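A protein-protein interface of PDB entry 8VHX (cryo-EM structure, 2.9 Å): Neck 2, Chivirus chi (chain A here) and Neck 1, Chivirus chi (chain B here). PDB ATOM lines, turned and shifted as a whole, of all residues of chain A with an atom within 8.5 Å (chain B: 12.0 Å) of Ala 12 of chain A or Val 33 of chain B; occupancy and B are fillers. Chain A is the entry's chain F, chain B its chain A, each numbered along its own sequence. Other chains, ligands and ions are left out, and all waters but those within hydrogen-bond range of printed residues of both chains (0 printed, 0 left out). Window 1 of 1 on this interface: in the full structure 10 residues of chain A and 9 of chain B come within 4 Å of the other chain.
OD2 of Asp 35 of chain B is in salt-bridge range of NZ of Lys 9 of chain A (3.2 Å). The guanidinium group (NH1) of Arg 13 of chain A is in salt-bridge range of the side-chain carboxylate (OD2) of Asp 35 of chain B (2.4 Å). The side-chain amide oxygen (OD1) of Asn 37 of chain B sits at hydrogen-bond distance from the guanidinium group (NH1) of Arg 13 of chain A (3.1 Å). ND2 of Asn 37 of chain B lies within hydrogen-bond range of OE2 of Glu 112 of chain A. The side-chain carboxylate of Glu 39 of chain B is in salt-bridge range of the guanidinium group of Arg 41 of chain A (3.6 Å). The side-chain carboxylate (OD2) of Asp 15 of chain A sits at hydrogen-bond distance from the side-chain hydroxyl (OH) of Tyr 43 of chain B (3.1 Å).
Of the 19 printed residues of chain A, 9 touch a printed residue of chain B. Hydrophobic or aromatic side chains of chain A that line the printed part of chain B: Ile 8, Ala 12 and Val 16. Hydrophobic or aromatic side chains of chain B that line the printed part of chain A: Val 30, Val 33, Val 41 and Tyr 43. Among the printed residues, 16 pairs touch across the chains.
Ile 8 of chain A touches just these residues of chain B: Val 30 (3.6 Å) and Val 33 (3.4 Å). No residue of chain B comes within 4 Å of Ala 10 of chain A. Of chain B, only Tyr 43 comes within 4 Å of Lys 11 of chain A. Printed residues of chain B within 4 Å of Ala 12 of chain A: Val 33 (3.98 Å), Val 41 (3.5 Å) and Tyr 43 (3.8 Å). Printed residues of chain B within 4 Å of Arg 13 of chain A: Asp 35 (2.4 Å), Asn 37 (3.1 Å) and Glu 39 (3.2 Å). Arg 14 of chain A touches none of the printed residues of chain B. Of the printed residues of chain B, Val 16 of chain A touches Arg 40 and Val 41. Of the printed residues of chain A, Val 33 of chain B touches Ile 8 and Ala 12. Of the printed residues of chain A, Asp 35 of chain B touches Lys 9 and Arg 13. Of the printed residues of chain A, Gln 36 of chain B touches Lys 9. Of the printed residues of chain A, Glu 39 of chain B touches Arg 13 (3.2 Å) and Arg 41 (3.6 Å). Printed residues of chain A within 4 Å of Arg 40 of chain B: Val 16 (3.97 Å). The nearest printed residue of chain A that does not touch Val 33 of chain B is Phe 5 of chain A (4.3 Å).
O of Arg 31 of chain B lies within hydrogen-bond range of N of Tyr 43 of chain B (2.7 Å). The guanidinium group (NH2) of Arg 40 of chain B lies within salt-bridge range of the side-chain carboxylate (OE2) of Glu 42 of chain B (3.1 Å). NZ of Lys 11 of chain A is in salt-bridge range of OD2 of Asp 15 of chain A (2.9 Å). O of Asp 15 of chain A sits at hydrogen-bond distance from OG of Ser 19 of chain A (3.1 Å). A ring nitrogen (ND1) of His 17 of chain A is in hydrogen-bond range of the guanidinium group of Arg 41 of chain A, at 3.0 Å. The guanidinium group (NH1) of Arg 41 of chain A is in salt-bridge range of the side-chain carboxylate (OE1) of Glu 112 of chain A (2.5 Å).
Among the printed residues, pairs that only touch across the chains: Ile 8 of chain A with Val 30 of chain B, Ile 8 of chain A with Val 33 of chain B, Lys 9 of chain A with Gln 36 of chain B, Lys 11 of chain A with Tyr 43 of chain B, Ala 12 of chain A with Val 33 of chain B, Ala 12 of chain A with Val 41 of chain B, Ala 12 of chain A with Tyr 43 of chain B, Arg 13 of chain A with Glu 39 of chain B, Val 16 of chain A with Arg 40 of chain B and Val 16 of chain A with Val 41 of chain B.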
ATOM      1  N   PHE A   5     -21.720 -19.770 -18.963  1.00  0.00           N
ATOM      2  CA  PHE A   5     -20.354 -19.968 -18.500  1.00  0.00           C
ATOM      3  C   PHE A   5     -20.009 -21.439 -18.360  1.00  0.00           C
ATOM      4  O   PHE A   5     -18.838 -21.814 -18.471  1.00  0.00           O
ATOM      5  CB  PHE A   5     -20.152 -19.268 -17.172  1.00  0.00           C
ATOM      6  CG  PHE A   5     -18.742 -19.262 -16.706  1.00  0.00           C
ATOM      7  CD1 PHE A   5     -17.775 -18.573 -17.398  1.00  0.00           C
ATOM      8  CD2 PHE A   5     -18.377 -19.949 -15.577  1.00  0.00           C
ATOM      9  CE1 PHE A   5     -16.488 -18.574 -16.970  1.00  0.00           C
ATOM     10  CE2 PHE A   5     -17.087 -19.946 -15.155  1.00  0.00           C
ATOM     11  CZ  PHE A   5     -16.143 -19.258 -15.854  1.00  0.00           C
ATOM     12  N   ALA A   6     -21.000 -22.283 -18.105  1.00  0.00           N
ATOM     13  CA  ALA A   6     -20.736 -23.706 -17.966  1.00  0.00           C
ATOM     14  C   ALA A   6     -20.193 -24.297 -19.256  1.00  0.00           C
ATOM     15  O   ALA A   6     -19.410 -25.251 -19.226  1.00  0.00           O
ATOM     16  CB  ALA A   6     -22.007 -24.426 -17.544  1.00  0.00           C
ATOM     17  N   ALA A   7     -20.615 -23.762 -20.399  1.00  0.00           N
ATOM     18  CA  ALA A   7     -20.108 -24.225 -21.682  1.00  0.00           C
ATOM     19  C   ALA A   7     -18.792 -23.562 -22.034  1.00  0.00           C
ATOM     20  O   ALA A   7     -17.907 -24.194 -22.619  1.00  0.00           O
ATOM     21  CB  ALA A   7     -21.125 -23.941 -22.767  1.00  0.00           C
ATOM     22  N   ILE A   8     -18.665 -22.283 -21.710  1.00  0.00           N
ATOM     23  CA  ILE A   8     -17.407 -21.581 -21.901  1.00  0.00           C
ATOM     24  C   ILE A   8     -16.297 -22.282 -21.142  1.00  0.00           C
ATOM     25  O   ILE A   8     -15.213 -22.533 -21.677  1.00  0.00           O
ATOM     26  CB  ILE A   8     -17.551 -20.122 -21.453  1.00  0.00           C
ATOM     27  CG1 ILE A   8     -18.504 -19.383 -22.369  1.00  0.00           C
ATOM     28  CG2 ILE A   8     -16.246 -19.469 -21.469  1.00  0.00           C
ATOM     29  CD1 ILE A   8     -19.034 -18.138 -21.780  1.00  0.00           C
ATOM     30  N   LYS A   9     -16.547 -22.586 -19.873  1.00  0.00           N
ATOM     31  CA  LYS A   9     -15.569 -23.296 -19.063  1.00  0.00           C
ATOM     32  C   LYS A   9     -15.212 -24.640 -19.674  1.00  0.00           C
ATOM     33  O   LYS A   9     -14.039 -25.030 -19.700  1.00  0.00           O
ATOM     34  CB  LYS A   9     -16.120 -23.475 -17.656  1.00  0.00           C
ATOM     35  CG  LYS A   9     -15.216 -24.225 -16.744  1.00  0.00           C
ATOM     36  CD  LYS A   9     -15.759 -24.330 -15.348  1.00  0.00           C
ATOM     37  CE  LYS A   9     -15.761 -23.003 -14.660  1.00  0.00           C
ATOM     38  NZ  LYS A   9     -15.484 -23.139 -13.203  1.00  0.00           N
ATOM     39  N   ALA A  10     -16.211 -25.364 -20.166  1.00  0.00           N
ATOM     40  CA  ALA A  10     -15.956 -26.663 -20.768  1.00  0.00           C
ATOM     41  C   ALA A  10     -15.057 -26.535 -21.981  1.00  0.00           C
ATOM     42  O   ALA A  10     -14.070 -27.262 -22.119  1.00  0.00           O
ATOM     43  CB  ALA A  10     -17.270 -27.319 -21.154  1.00  0.00           C
ATOM     44  N   LYS A  11     -15.402 -25.633 -22.892  1.00  0.00           N
ATOM     45  CA  LYS A  11     -14.590 -25.442 -24.082  1.00  0.00           C
ATOM     46  C   LYS A  11     -13.184 -24.993 -23.724  1.00  0.00           C
ATOM     47  O   LYS A  11     -12.211 -25.396 -24.367  1.00  0.00           O
ATOM     48  CB  LYS A  11     -15.260 -24.433 -24.997  1.00  0.00           C
ATOM     49  CG  LYS A  11     -14.448 -24.107 -26.192  1.00  0.00           C
ATOM     50  CD  LYS A  11     -15.200 -23.233 -27.131  1.00  0.00           C
ATOM     51  CE  LYS A  11     -14.238 -22.495 -28.020  1.00  0.00           C
ATOM     52  NZ  LYS A  11     -13.217 -23.403 -28.594  1.00  0.00           N
ATOM     53  N   ALA A  12     -13.060 -24.148 -22.707  1.00  0.00           N
ATOM     54  CA  ALA A  12     -11.750 -23.711 -22.254  1.00  0.00           C
ATOM     55  C   ALA A  12     -10.906 -24.885 -21.795  1.00  0.00           C
ATOM     56  O   ALA A  12      -9.744 -25.022 -22.189  1.00  0.00           O
ATOM     57  CB  ALA A  12     -11.919 -22.706 -21.129  1.00  0.00           C
ATOM     58  N   ARG A  13     -11.467 -25.729 -20.936  1.00  0.00           N
ATOM     59  CA  ARG A  13     -10.735 -26.888 -20.452  1.00  0.00           C
ATOM     60  C   ARG A  13     -10.405 -27.846 -21.588  1.00  0.00           C
ATOM     61  O   ARG A  13      -9.320 -28.438 -21.622  1.00  0.00           O
ATOM     62  CB  ARG A  13     -11.556 -27.578 -19.377  1.00  0.00           C
ATOM     63  CG  ARG A  13     -11.772 -26.721 -18.165  1.00  0.00           C
ATOM     64  CD  ARG A  13     -12.446 -27.465 -17.060  1.00  0.00           C
ATOM     65  NE  ARG A  13     -12.651 -26.628 -15.888  1.00  0.00           N
ATOM     66  CZ  ARG A  13     -12.911 -27.105 -14.680  1.00  0.00           C
ATOM     67  NH1 ARG A  13     -13.088 -26.285 -13.664  1.00  0.00           N
ATOM     68  NH2 ARG A  13     -12.988 -28.407 -14.489  1.00  0.00           N
ATOM     69  N   ARG A  14     -11.320 -27.988 -22.543  1.00  0.00           N
ATOM     70  CA  ARG A  14     -11.085 -28.862 -23.682  1.00  0.00           C
ATOM     71  C   ARG A  14      -9.930 -28.363 -24.532  1.00  0.00           C
ATOM     72  O   ARG A  14      -9.105 -29.155 -25.000  1.00  0.00           O
ATOM     73  CB  ARG A  14     -12.358 -28.973 -24.511  1.00  0.00           C
ATOM     74  CG  ARG A  14     -13.358 -29.931 -23.935  1.00  0.00           C
ATOM     75  CD  ARG A  14     -14.527 -30.199 -24.846  1.00  0.00           C
ATOM     76  NE  ARG A  14     -15.630 -29.262 -24.694  1.00  0.00           N
ATOM     77  CZ  ARG A  14     -15.952 -28.319 -25.572  1.00  0.00           C
ATOM     78  NH1 ARG A  14     -16.981 -27.527 -25.331  1.00  0.00           N
ATOM     79  NH2 ARG A  14     -15.258 -28.153 -26.688  1.00  0.00           N
ATOM     80  N   ASP A  15      -9.846 -27.052 -24.735  1.00  0.00           N
ATOM     81  CA  ASP A  15      -8.750 -26.496 -25.514  1.00  0.00           C
ATOM     82  C   ASP A  15      -7.438 -26.549 -24.752  1.00  0.00           C
ATOM     83  O   ASP A  15      -6.386 -26.823 -25.341  1.00  0.00           O
ATOM     84  CB  ASP A  15      -9.081 -25.069 -25.903  1.00  0.00           C
ATOM     85  CG  ASP A  15     -10.273 -24.986 -26.824  1.00  0.00           C
ATOM     86  OD1 ASP A  15     -10.633 -26.022 -27.415  1.00  0.00           O
ATOM     87  OD2 ASP A  15     -10.850 -23.890 -26.968  1.00  0.00           O
ATOM     88  N   VAL A  16      -7.486 -26.323 -23.443  1.00  0.00           N
ATOM     89  CA  VAL A  16      -6.300 -26.474 -22.611  1.00  0.00           C
ATOM     90  C   VAL A  16      -5.742 -27.880 -22.740  1.00  0.00           C
ATOM     91  O   VAL A  16      -4.529 -28.081 -22.856  1.00  0.00           O
ATOM     92  CB  VAL A  16      -6.624 -26.142 -21.147  1.00  0.00           C
ATOM     93  CG1 VAL A  16      -5.487 -26.469 -20.295  1.00  0.00           C
ATOM     94  CG2 VAL A  16      -6.927 -24.706 -20.985  1.00  0.00           C
ATOM     95  N   HIS A  17      -6.619 -28.876 -22.701  1.00  0.00           N
ATOM     96  CA  HIS A  17      -6.164 -30.246 -22.848  1.00  0.00           C
ATOM     97  C   HIS A  17      -5.639 -30.515 -24.246  1.00  0.00           C
ATOM     98  O   HIS A  17      -4.556 -31.080 -24.410  1.00  0.00           O
ATOM     99  CB  HIS A  17      -7.295 -31.203 -22.521  1.00  0.00           C
ATOM    100  CG  HIS A  17      -6.828 -32.526 -22.016  1.00  0.00           C
ATOM    101  ND1 HIS A  17      -6.394 -32.712 -20.725  1.00  0.00           N
ATOM    102  CD2 HIS A  17      -6.715 -33.724 -22.630  1.00  0.00           C
ATOM    103  CE1 HIS A  17      -6.033 -33.970 -20.565  1.00  0.00           C
ATOM    104  NE2 HIS A  17      -6.219 -34.606 -21.705  1.00  0.00           N
ATOM    105  N   ALA A  18      -6.384 -30.115 -25.268  1.00  0.00           N
ATOM    106  CA  ALA A  18      -5.947 -30.350 -26.631  1.00  0.00           C
ATOM    107  C   ALA A  18      -4.610 -29.702 -26.922  1.00  0.00           C
ATOM    108  O   ALA A  18      -3.912 -30.126 -27.847  1.00  0.00           O
ATOM    109  CB  ALA A  18      -6.996 -29.828 -27.595  1.00  0.00           C
ATOM    110  N   SER A  19      -4.240 -28.679 -26.166  1.00  0.00           N
ATOM    111  CA  SER A  19      -2.969 -28.017 -26.393  1.00  0.00           C
ATOM    112  C   SER A  19      -1.842 -28.557 -25.524  1.00  0.00           C
ATOM    113  O   SER A  19      -0.707 -28.665 -25.992  1.00  0.00           O
ATOM    114  CB  SER A  19      -3.124 -26.523 -26.159  1.00  0.00           C
ATOM    115  OG  SER A  19      -4.029 -25.963 -27.086  1.00  0.00           O
ATOM    116  N   ARG A  41      -2.589 -34.801 -18.804  1.00  0.00           N
ATOM    117  CA  ARG A  41      -1.699 -33.737 -18.378  1.00  0.00           C
ATOM    118  C   ARG A  41      -1.064 -34.133 -17.057  1.00  0.00           C
ATOM    119  O   ARG A  41      -1.772 -34.429 -16.092  1.00  0.00           O
ATOM    120  CB  ARG A  41      -2.444 -32.423 -18.211  1.00  0.00           C
ATOM    121  CG  ARG A  41      -2.728 -31.690 -19.457  1.00  0.00           C
ATOM    122  CD  ARG A  41      -3.477 -30.439 -19.161  1.00  0.00           C
ATOM    123  NE  ARG A  41      -4.906 -30.644 -19.087  1.00  0.00           N
ATOM    124  CZ  ARG A  41      -5.718 -29.900 -18.357  1.00  0.00           C
ATOM    125  NH1 ARG A  41      -7.015 -30.141 -18.355  1.00  0.00           N
ATOM    126  NH2 ARG A  41      -5.231 -28.911 -17.634  1.00  0.00           N
ATOM    127  N   PRO A 110     -16.898 -29.507 -15.703  1.00  0.00           N
ATOM    128  CA  PRO A 110     -17.607 -30.290 -16.712  1.00  0.00           C
ATOM    129  C   PRO A 110     -16.762 -31.215 -17.576  1.00  0.00           C
ATOM    130  O   PRO A 110     -17.327 -32.071 -18.265  1.00  0.00           O
ATOM    131  CB  PRO A 110     -18.235 -29.192 -17.568  1.00  0.00           C
ATOM    132  CG  PRO A 110     -17.253 -28.154 -17.516  1.00  0.00           C
ATOM    133  CD  PRO A 110     -16.742 -28.120 -16.141  1.00  0.00           C
ATOM    134  N   VAL A 111     -15.438 -31.068 -17.588  1.00  0.00           N
ATOM    135  CA  VAL A 111     -14.659 -31.727 -18.629  1.00  0.00           C
ATOM    136  C   VAL A 111     -13.622 -32.695 -18.096  1.00  0.00           C
ATOM    137  O   VAL A 111     -13.334 -33.711 -18.736  1.00  0.00           O
ATOM    138  CB  VAL A 111     -13.959 -30.683 -19.506  1.00  0.00           C
ATOM    139  CG1 VAL A 111     -12.862 -31.313 -20.282  1.00  0.00           C
ATOM    140  CG2 VAL A 111     -14.920 -30.094 -20.441  1.00  0.00           C
ATOM    141  N   GLU A 112     -13.055 -32.409 -16.937  1.00  0.00           N
ATOM    142  CA  GLU A 112     -11.852 -33.101 -16.522  1.00  0.00           C
ATOM    143  C   GLU A 112     -12.004 -33.683 -15.132  1.00  0.00           C
ATOM    144  O   GLU A 112     -12.784 -33.210 -14.303  1.00  0.00           O
ATOM    145  CB  GLU A 112     -10.637 -32.174 -16.568  1.00  0.00           C
ATOM    146  CG  GLU A 112     -10.699 -31.003 -15.628  1.00  0.00           C
ATOM    147  CD  GLU A 112      -9.485 -30.113 -15.736  1.00  0.00           C
ATOM    148  OE1 GLU A 112      -8.961 -29.960 -16.857  1.00  0.00           O
ATOM    149  OE2 GLU A 112      -9.055 -29.565 -14.702  1.00  0.00           O
ATOM    150  N   GLY B  27     -21.650  -8.085 -27.516  1.00  0.00           N
ATOM    151  CA  GLY B  27     -20.527  -8.012 -26.611  1.00  0.00           C
ATOM    152  C   GLY B  27     -20.425  -9.162 -25.645  1.00  0.00           C
ATOM    153  O   GLY B  27     -19.972  -8.973 -24.514  1.00  0.00           O
ATOM    154  N   GLY B  28     -20.841 -10.349 -26.056  1.00  0.00           N
ATOM    155  CA  GLY B  28     -20.741 -11.527 -25.230  1.00  0.00           C
ATOM    156  C   GLY B  28     -19.879 -12.601 -25.852  1.00  0.00           C
ATOM    157  O   GLY B  28     -20.006 -13.778 -25.505  1.00  0.00           O
ATOM    158  N   SER B  29     -19.006 -12.214 -26.774  1.00  0.00           N
ATOM    159  CA  SER B  29     -18.096 -13.148 -27.419  1.00  0.00           C
ATOM    160  C   SER B  29     -16.832 -13.248 -26.588  1.00  0.00           C
ATOM    161  O   SER B  29     -16.200 -12.233 -26.281  1.00  0.00           O
ATOM    162  CB  SER B  29     -17.761 -12.711 -28.838  1.00  0.00           C
ATOM    163  OG  SER B  29     -16.869 -13.618 -29.446  1.00  0.00           O
ATOM    164  N   VAL B  30     -16.466 -14.473 -26.232  1.00  0.00           N
ATOM    165  CA  VAL B  30     -15.404 -14.687 -25.272  1.00  0.00           C
ATOM    166  C   VAL B  30     -14.050 -14.554 -25.943  1.00  0.00           C
ATOM    167  O   VAL B  30     -13.805 -15.101 -27.025  1.00  0.00           O
ATOM    168  CB  VAL B  30     -15.581 -16.058 -24.615  1.00  0.00           C
ATOM    169  CG1 VAL B  30     -14.468 -16.324 -23.688  1.00  0.00           C
ATOM    170  CG2 VAL B  30     -16.874 -16.086 -23.885  1.00  0.00           C
ATOM    171  N   ARG B  31     -13.172 -13.814 -25.298  1.00  0.00           N
ATOM    172  CA  ARG B  31     -11.799 -13.638 -25.715  1.00  0.00           C
ATOM    173  C   ARG B  31     -10.821 -14.151 -24.682  1.00  0.00           C
ATOM    174  O   ARG B  31      -9.692 -14.489 -25.029  1.00  0.00           O
ATOM    175  CB  ARG B  31     -11.532 -12.157 -25.995  1.00  0.00           C
ATOM    176  CG  ARG B  31     -10.230 -11.822 -26.670  1.00  0.00           C
ATOM    177  CD  ARG B  31     -10.122 -10.332 -26.870  1.00  0.00           C
ATOM    178  NE  ARG B  31     -10.463  -9.610 -25.647  1.00  0.00           N
ATOM    179  CZ  ARG B  31      -9.692  -9.536 -24.568  1.00  0.00           C
ATOM    180  NH1 ARG B  31     -10.118  -8.860 -23.511  1.00  0.00           N
ATOM    181  NH2 ARG B  31      -8.497 -10.117 -24.542  1.00  0.00           N
ATOM    182  N   VAL B  32     -11.234 -14.229 -23.425  1.00  0.00           N
ATOM    183  CA  VAL B  32     -10.427 -14.772 -22.345  1.00  0.00           C
ATOM    184  C   VAL B  32     -11.323 -15.540 -21.396  1.00  0.00           C
ATOM    185  O   VAL B  32     -12.455 -15.132 -21.127  1.00  0.00           O
ATOM    186  CB  VAL B  32      -9.688 -13.677 -21.567  1.00  0.00           C
ATOM    187  CG1 VAL B  32      -8.869 -14.296 -20.504  1.00  0.00           C
ATOM    188  CG2 VAL B  32      -8.853 -12.868 -22.487  1.00  0.00           C
ATOM    189  N   VAL B  33     -10.810 -16.648 -20.882  1.00  0.00           N
ATOM    190  CA  VAL B  33     -11.479 -17.425 -19.853  1.00  0.00           C
ATOM    191  C   VAL B  33     -10.455 -17.856 -18.824  1.00  0.00           C
ATOM    192  O   VAL B  33      -9.343 -18.264 -19.167  1.00  0.00           O
ATOM    193  CB  VAL B  33     -12.191 -18.651 -20.430  1.00  0.00           C
ATOM    194  CG1 VAL B  33     -13.008 -19.289 -19.393  1.00  0.00           C
ATOM    195  CG2 VAL B  33     -13.056 -18.238 -21.516  1.00  0.00           C
ATOM    196  N   VAL B  34     -10.839 -17.765 -17.562  1.00  0.00           N
ATOM    197  CA  VAL B  34     -10.032 -18.236 -16.453  1.00  0.00           C
ATOM    198  C   VAL B  34     -10.950 -18.984 -15.509  1.00  0.00           C
ATOM    199  O   VAL B  34     -12.036 -18.499 -15.180  1.00  0.00           O
ATOM    200  CB  VAL B  34      -9.327 -17.084 -15.725  1.00  0.00           C
ATOM    201  CG1 VAL B  34      -8.267 -17.604 -14.842  1.00  0.00           C
ATOM    202  CG2 VAL B  34      -8.736 -16.136 -16.698  1.00  0.00           C
ATOM    203  N   ASP B  35     -10.525 -20.159 -15.090  1.00  0.00           N
ATOM    204  CA  ASP B  35     -11.279 -20.959 -14.147  1.00  0.00           C
ATOM    205  C   ASP B  35     -10.651 -20.851 -12.767  1.00  0.00           C
ATOM    206  O   ASP B  35      -9.475 -20.517 -12.618  1.00  0.00           O
ATOM    207  CB  ASP B  35     -11.316 -22.412 -14.606  1.00  0.00           C
ATOM    208  CG  ASP B  35     -12.589 -23.109 -14.226  1.00  0.00           C
ATOM    209  OD1 ASP B  35     -13.299 -22.615 -13.326  1.00  0.00           O
ATOM    210  OD2 ASP B  35     -12.889 -24.153 -14.836  1.00  0.00           O
ATOM    211  N   GLN B  36     -11.455 -21.145 -11.749  1.00  0.00           N
ATOM    212  CA  GLN B  36     -10.933 -21.203 -10.393  1.00  0.00           C
ATOM    213  C   GLN B  36      -9.843 -22.253 -10.251  1.00  0.00           C
ATOM    214  O   GLN B  36      -9.134 -22.261  -9.239  1.00  0.00           O
ATOM    215  CB  GLN B  36     -12.084 -21.461  -9.430  1.00  0.00           C
ATOM    216  CG  GLN B  36     -12.772 -22.777  -9.620  1.00  0.00           C
ATOM    217  CD  GLN B  36     -14.164 -22.772  -9.057  1.00  0.00           C
ATOM    218  OE1 GLN B  36     -14.526 -21.893  -8.285  1.00  0.00           O
ATOM    219  NE2 GLN B  36     -14.965 -23.740  -9.463  1.00  0.00           N
ATOM    220  N   ASN B  37      -9.689 -23.128 -11.244  1.00  0.00           N
ATOM    221  CA  ASN B  37      -8.521 -23.986 -11.360  1.00  0.00           C
ATOM    222  C   ASN B  37      -7.243 -23.211 -11.630  1.00  0.00           C
ATOM    223  O   ASN B  37      -6.169 -23.817 -11.654  1.00  0.00           O
ATOM    224  CB  ASN B  37      -8.741 -24.982 -12.486  1.00  0.00           C
ATOM    225  CG  ASN B  37      -9.817 -25.969 -12.180  1.00  0.00           C
ATOM    226  OD1 ASN B  37     -10.837 -25.629 -11.588  1.00  0.00           O
ATOM    227  ND2 ASN B  37      -9.604 -27.209 -12.584  1.00  0.00           N
ATOM    228  N   SER B  38      -7.332 -21.901 -11.851  1.00  0.00           N
ATOM    229  CA  SER B  38      -6.183 -21.059 -12.179  1.00  0.00           C
ATOM    230  C   SER B  38      -5.631 -21.372 -13.561  1.00  0.00           C
ATOM    231  O   SER B  38      -4.466 -21.096 -13.851  1.00  0.00           O
ATOM    232  CB  SER B  38      -5.075 -21.183 -11.132  1.00  0.00           C
ATOM    233  OG  SER B  38      -3.959 -20.390 -11.491  1.00  0.00           O
ATOM    234  N   GLU B  39      -6.462 -21.925 -14.431  1.00  0.00           N
ATOM    235  CA  GLU B  39      -6.076 -22.217 -15.798  1.00  0.00           C
ATOM    236  C   GLU B  39      -6.804 -21.285 -16.750  1.00  0.00           C
ATOM    237  O   GLU B  39      -7.981 -20.976 -16.559  1.00  0.00           O
ATOM    238  CB  GLU B  39      -6.346 -23.676 -16.152  1.00  0.00           C
ATOM    239  CG  GLU B  39      -7.770 -24.067 -16.275  1.00  0.00           C
ATOM    240  CD  GLU B  39      -7.914 -25.548 -16.521  1.00  0.00           C
ATOM    241  OE1 GLU B  39      -7.081 -26.321 -16.010  1.00  0.00           O
ATOM    242  OE2 GLU B  39      -8.852 -25.943 -17.230  1.00  0.00           O
ATOM    243  N   ARG B  40      -6.094 -20.860 -17.785  1.00  0.00           N
ATOM    244  CA  ARG B  40      -6.468 -19.715 -18.590  1.00  0.00           C
ATOM    245  C   ARG B  40      -6.478 -20.096 -20.053  1.00  0.00           C
ATOM    246  O   ARG B  40      -5.718 -20.961 -20.487  1.00  0.00           O
ATOM    247  CB  ARG B  40      -5.513 -18.554 -18.375  1.00  0.00           C
ATOM    248  CG  ARG B  40      -5.680 -17.449 -19.347  1.00  0.00           C
ATOM    249  CD  ARG B  40      -4.671 -16.372 -19.150  1.00  0.00           C
ATOM    250  NE  ARG B  40      -4.964 -15.559 -17.979  1.00  0.00           N
ATOM    251  CZ  ARG B  40      -5.347 -14.292 -18.021  1.00  0.00           C
ATOM    252  NH1 ARG B  40      -5.576 -13.649 -16.896  1.00  0.00           N
ATOM    253  NH2 ARG B  40      -5.531 -13.672 -19.176  1.00  0.00           N
ATOM    254  N   VAL B  41      -7.358 -19.449 -20.803  1.00  0.00           N
ATOM    255  CA  VAL B  41      -7.454 -19.624 -22.240  1.00  0.00           C
ATOM    256  C   VAL B  41      -7.786 -18.280 -22.854  1.00  0.00           C
ATOM    257  O   VAL B  41      -8.786 -17.658 -22.488  1.00  0.00           O
ATOM    258  CB  VAL B  41      -8.517 -20.662 -22.616  1.00  0.00           C
ATOM    259  CG1 VAL B  41      -8.396 -21.041 -24.038  1.00  0.00           C
ATOM    260  CG2 VAL B  41      -8.381 -21.862 -21.766  1.00  0.00           C
ATOM    261  N   GLU B  42      -6.968 -17.850 -23.799  1.00  0.00           N
ATOM    262  CA  GLU B  42      -7.207 -16.636 -24.553  1.00  0.00           C
ATOM    263  C   GLU B  42      -7.470 -17.010 -25.996  1.00  0.00           C
ATOM    264  O   GLU B  42      -6.834 -17.914 -26.539  1.00  0.00           O
ATOM    265  CB  GLU B  42      -6.035 -15.682 -24.475  1.00  0.00           C
ATOM    266  CG  GLU B  42      -5.562 -15.405 -23.081  1.00  0.00           C
ATOM    267  CD  GLU B  42      -4.666 -14.194 -22.998  1.00  0.00           C
ATOM    268  OE1 GLU B  42      -4.488 -13.512 -24.025  1.00  0.00           O
ATOM    269  OE2 GLU B  42      -4.130 -13.926 -21.902  1.00  0.00           O
ATOM    270  N   TYR B  43      -8.409 -16.311 -26.606  1.00  0.00           N
ATOM    271  CA  TYR B  43      -8.864 -16.610 -27.948  1.00  0.00           C
ATOM    272  C   TYR B  43      -8.536 -15.460 -28.882  1.00  0.00           C
ATOM    273  O   TYR B  43      -8.521 -14.296 -28.476  1.00  0.00           O
ATOM    274  CB  TYR B  43     -10.348 -16.852 -27.972  1.00  0.00           C
ATOM    275  CG  TYR B  43     -10.781 -18.093 -27.263  1.00  0.00           C
ATOM    276  CD1 TYR B  43     -10.623 -19.328 -27.840  1.00  0.00           C
ATOM    277  CD2 TYR B  43     -11.352 -18.030 -26.018  1.00  0.00           C
ATOM    278  CE1 TYR B  43     -11.019 -20.454 -27.198  1.00  0.00           C
ATOM    279  CE2 TYR B  43     -11.746 -19.150 -25.375  1.00  0.00           C
ATOM    280  CZ  TYR B  43     -11.577 -20.361 -25.969  1.00  0.00           C
ATOM    281  OH  TYR B  43     -11.968 -21.506 -25.344  1.00  0.00           O
ATOM    282  N   THR B  44      -8.277 -15.799 -30.137  1.00  0.00           N
ATOM    283  CA  THR B  44      -8.194 -14.781 -31.166  1.00  0.00           C
ATOM    284  C   THR B  44      -9.558 -14.136 -31.343  1.00  0.00           C
ATOM    285  O   THR B  44     -10.568 -14.821 -31.505  1.00  0.00           O
ATOM    286  CB  THR B  44      -7.717 -15.382 -32.478  1.00  0.00           C
ATOM    287  OG1 THR B  44      -6.442 -15.990 -32.287  1.00  0.00           O
ATOM    288  CG2 THR B  44      -7.576 -14.321 -33.501  1.00  0.00           C
ATOM    289  N   ALA B  45      -9.582 -12.813 -31.305  1.00  0.00           N
ATOM    290  CA  ALA B  45     -10.839 -12.096 -31.329  1.00  0.00           C
ATOM    291  C   ALA B  45     -11.593 -12.362 -32.617  1.00  0.00           C
ATOM    292  O   ALA B  45     -11.013 -12.388 -33.705  1.00  0.00           O
ATOM    293  CB  ALA B  45     -10.592 -10.608 -31.165  1.00  0.00           C
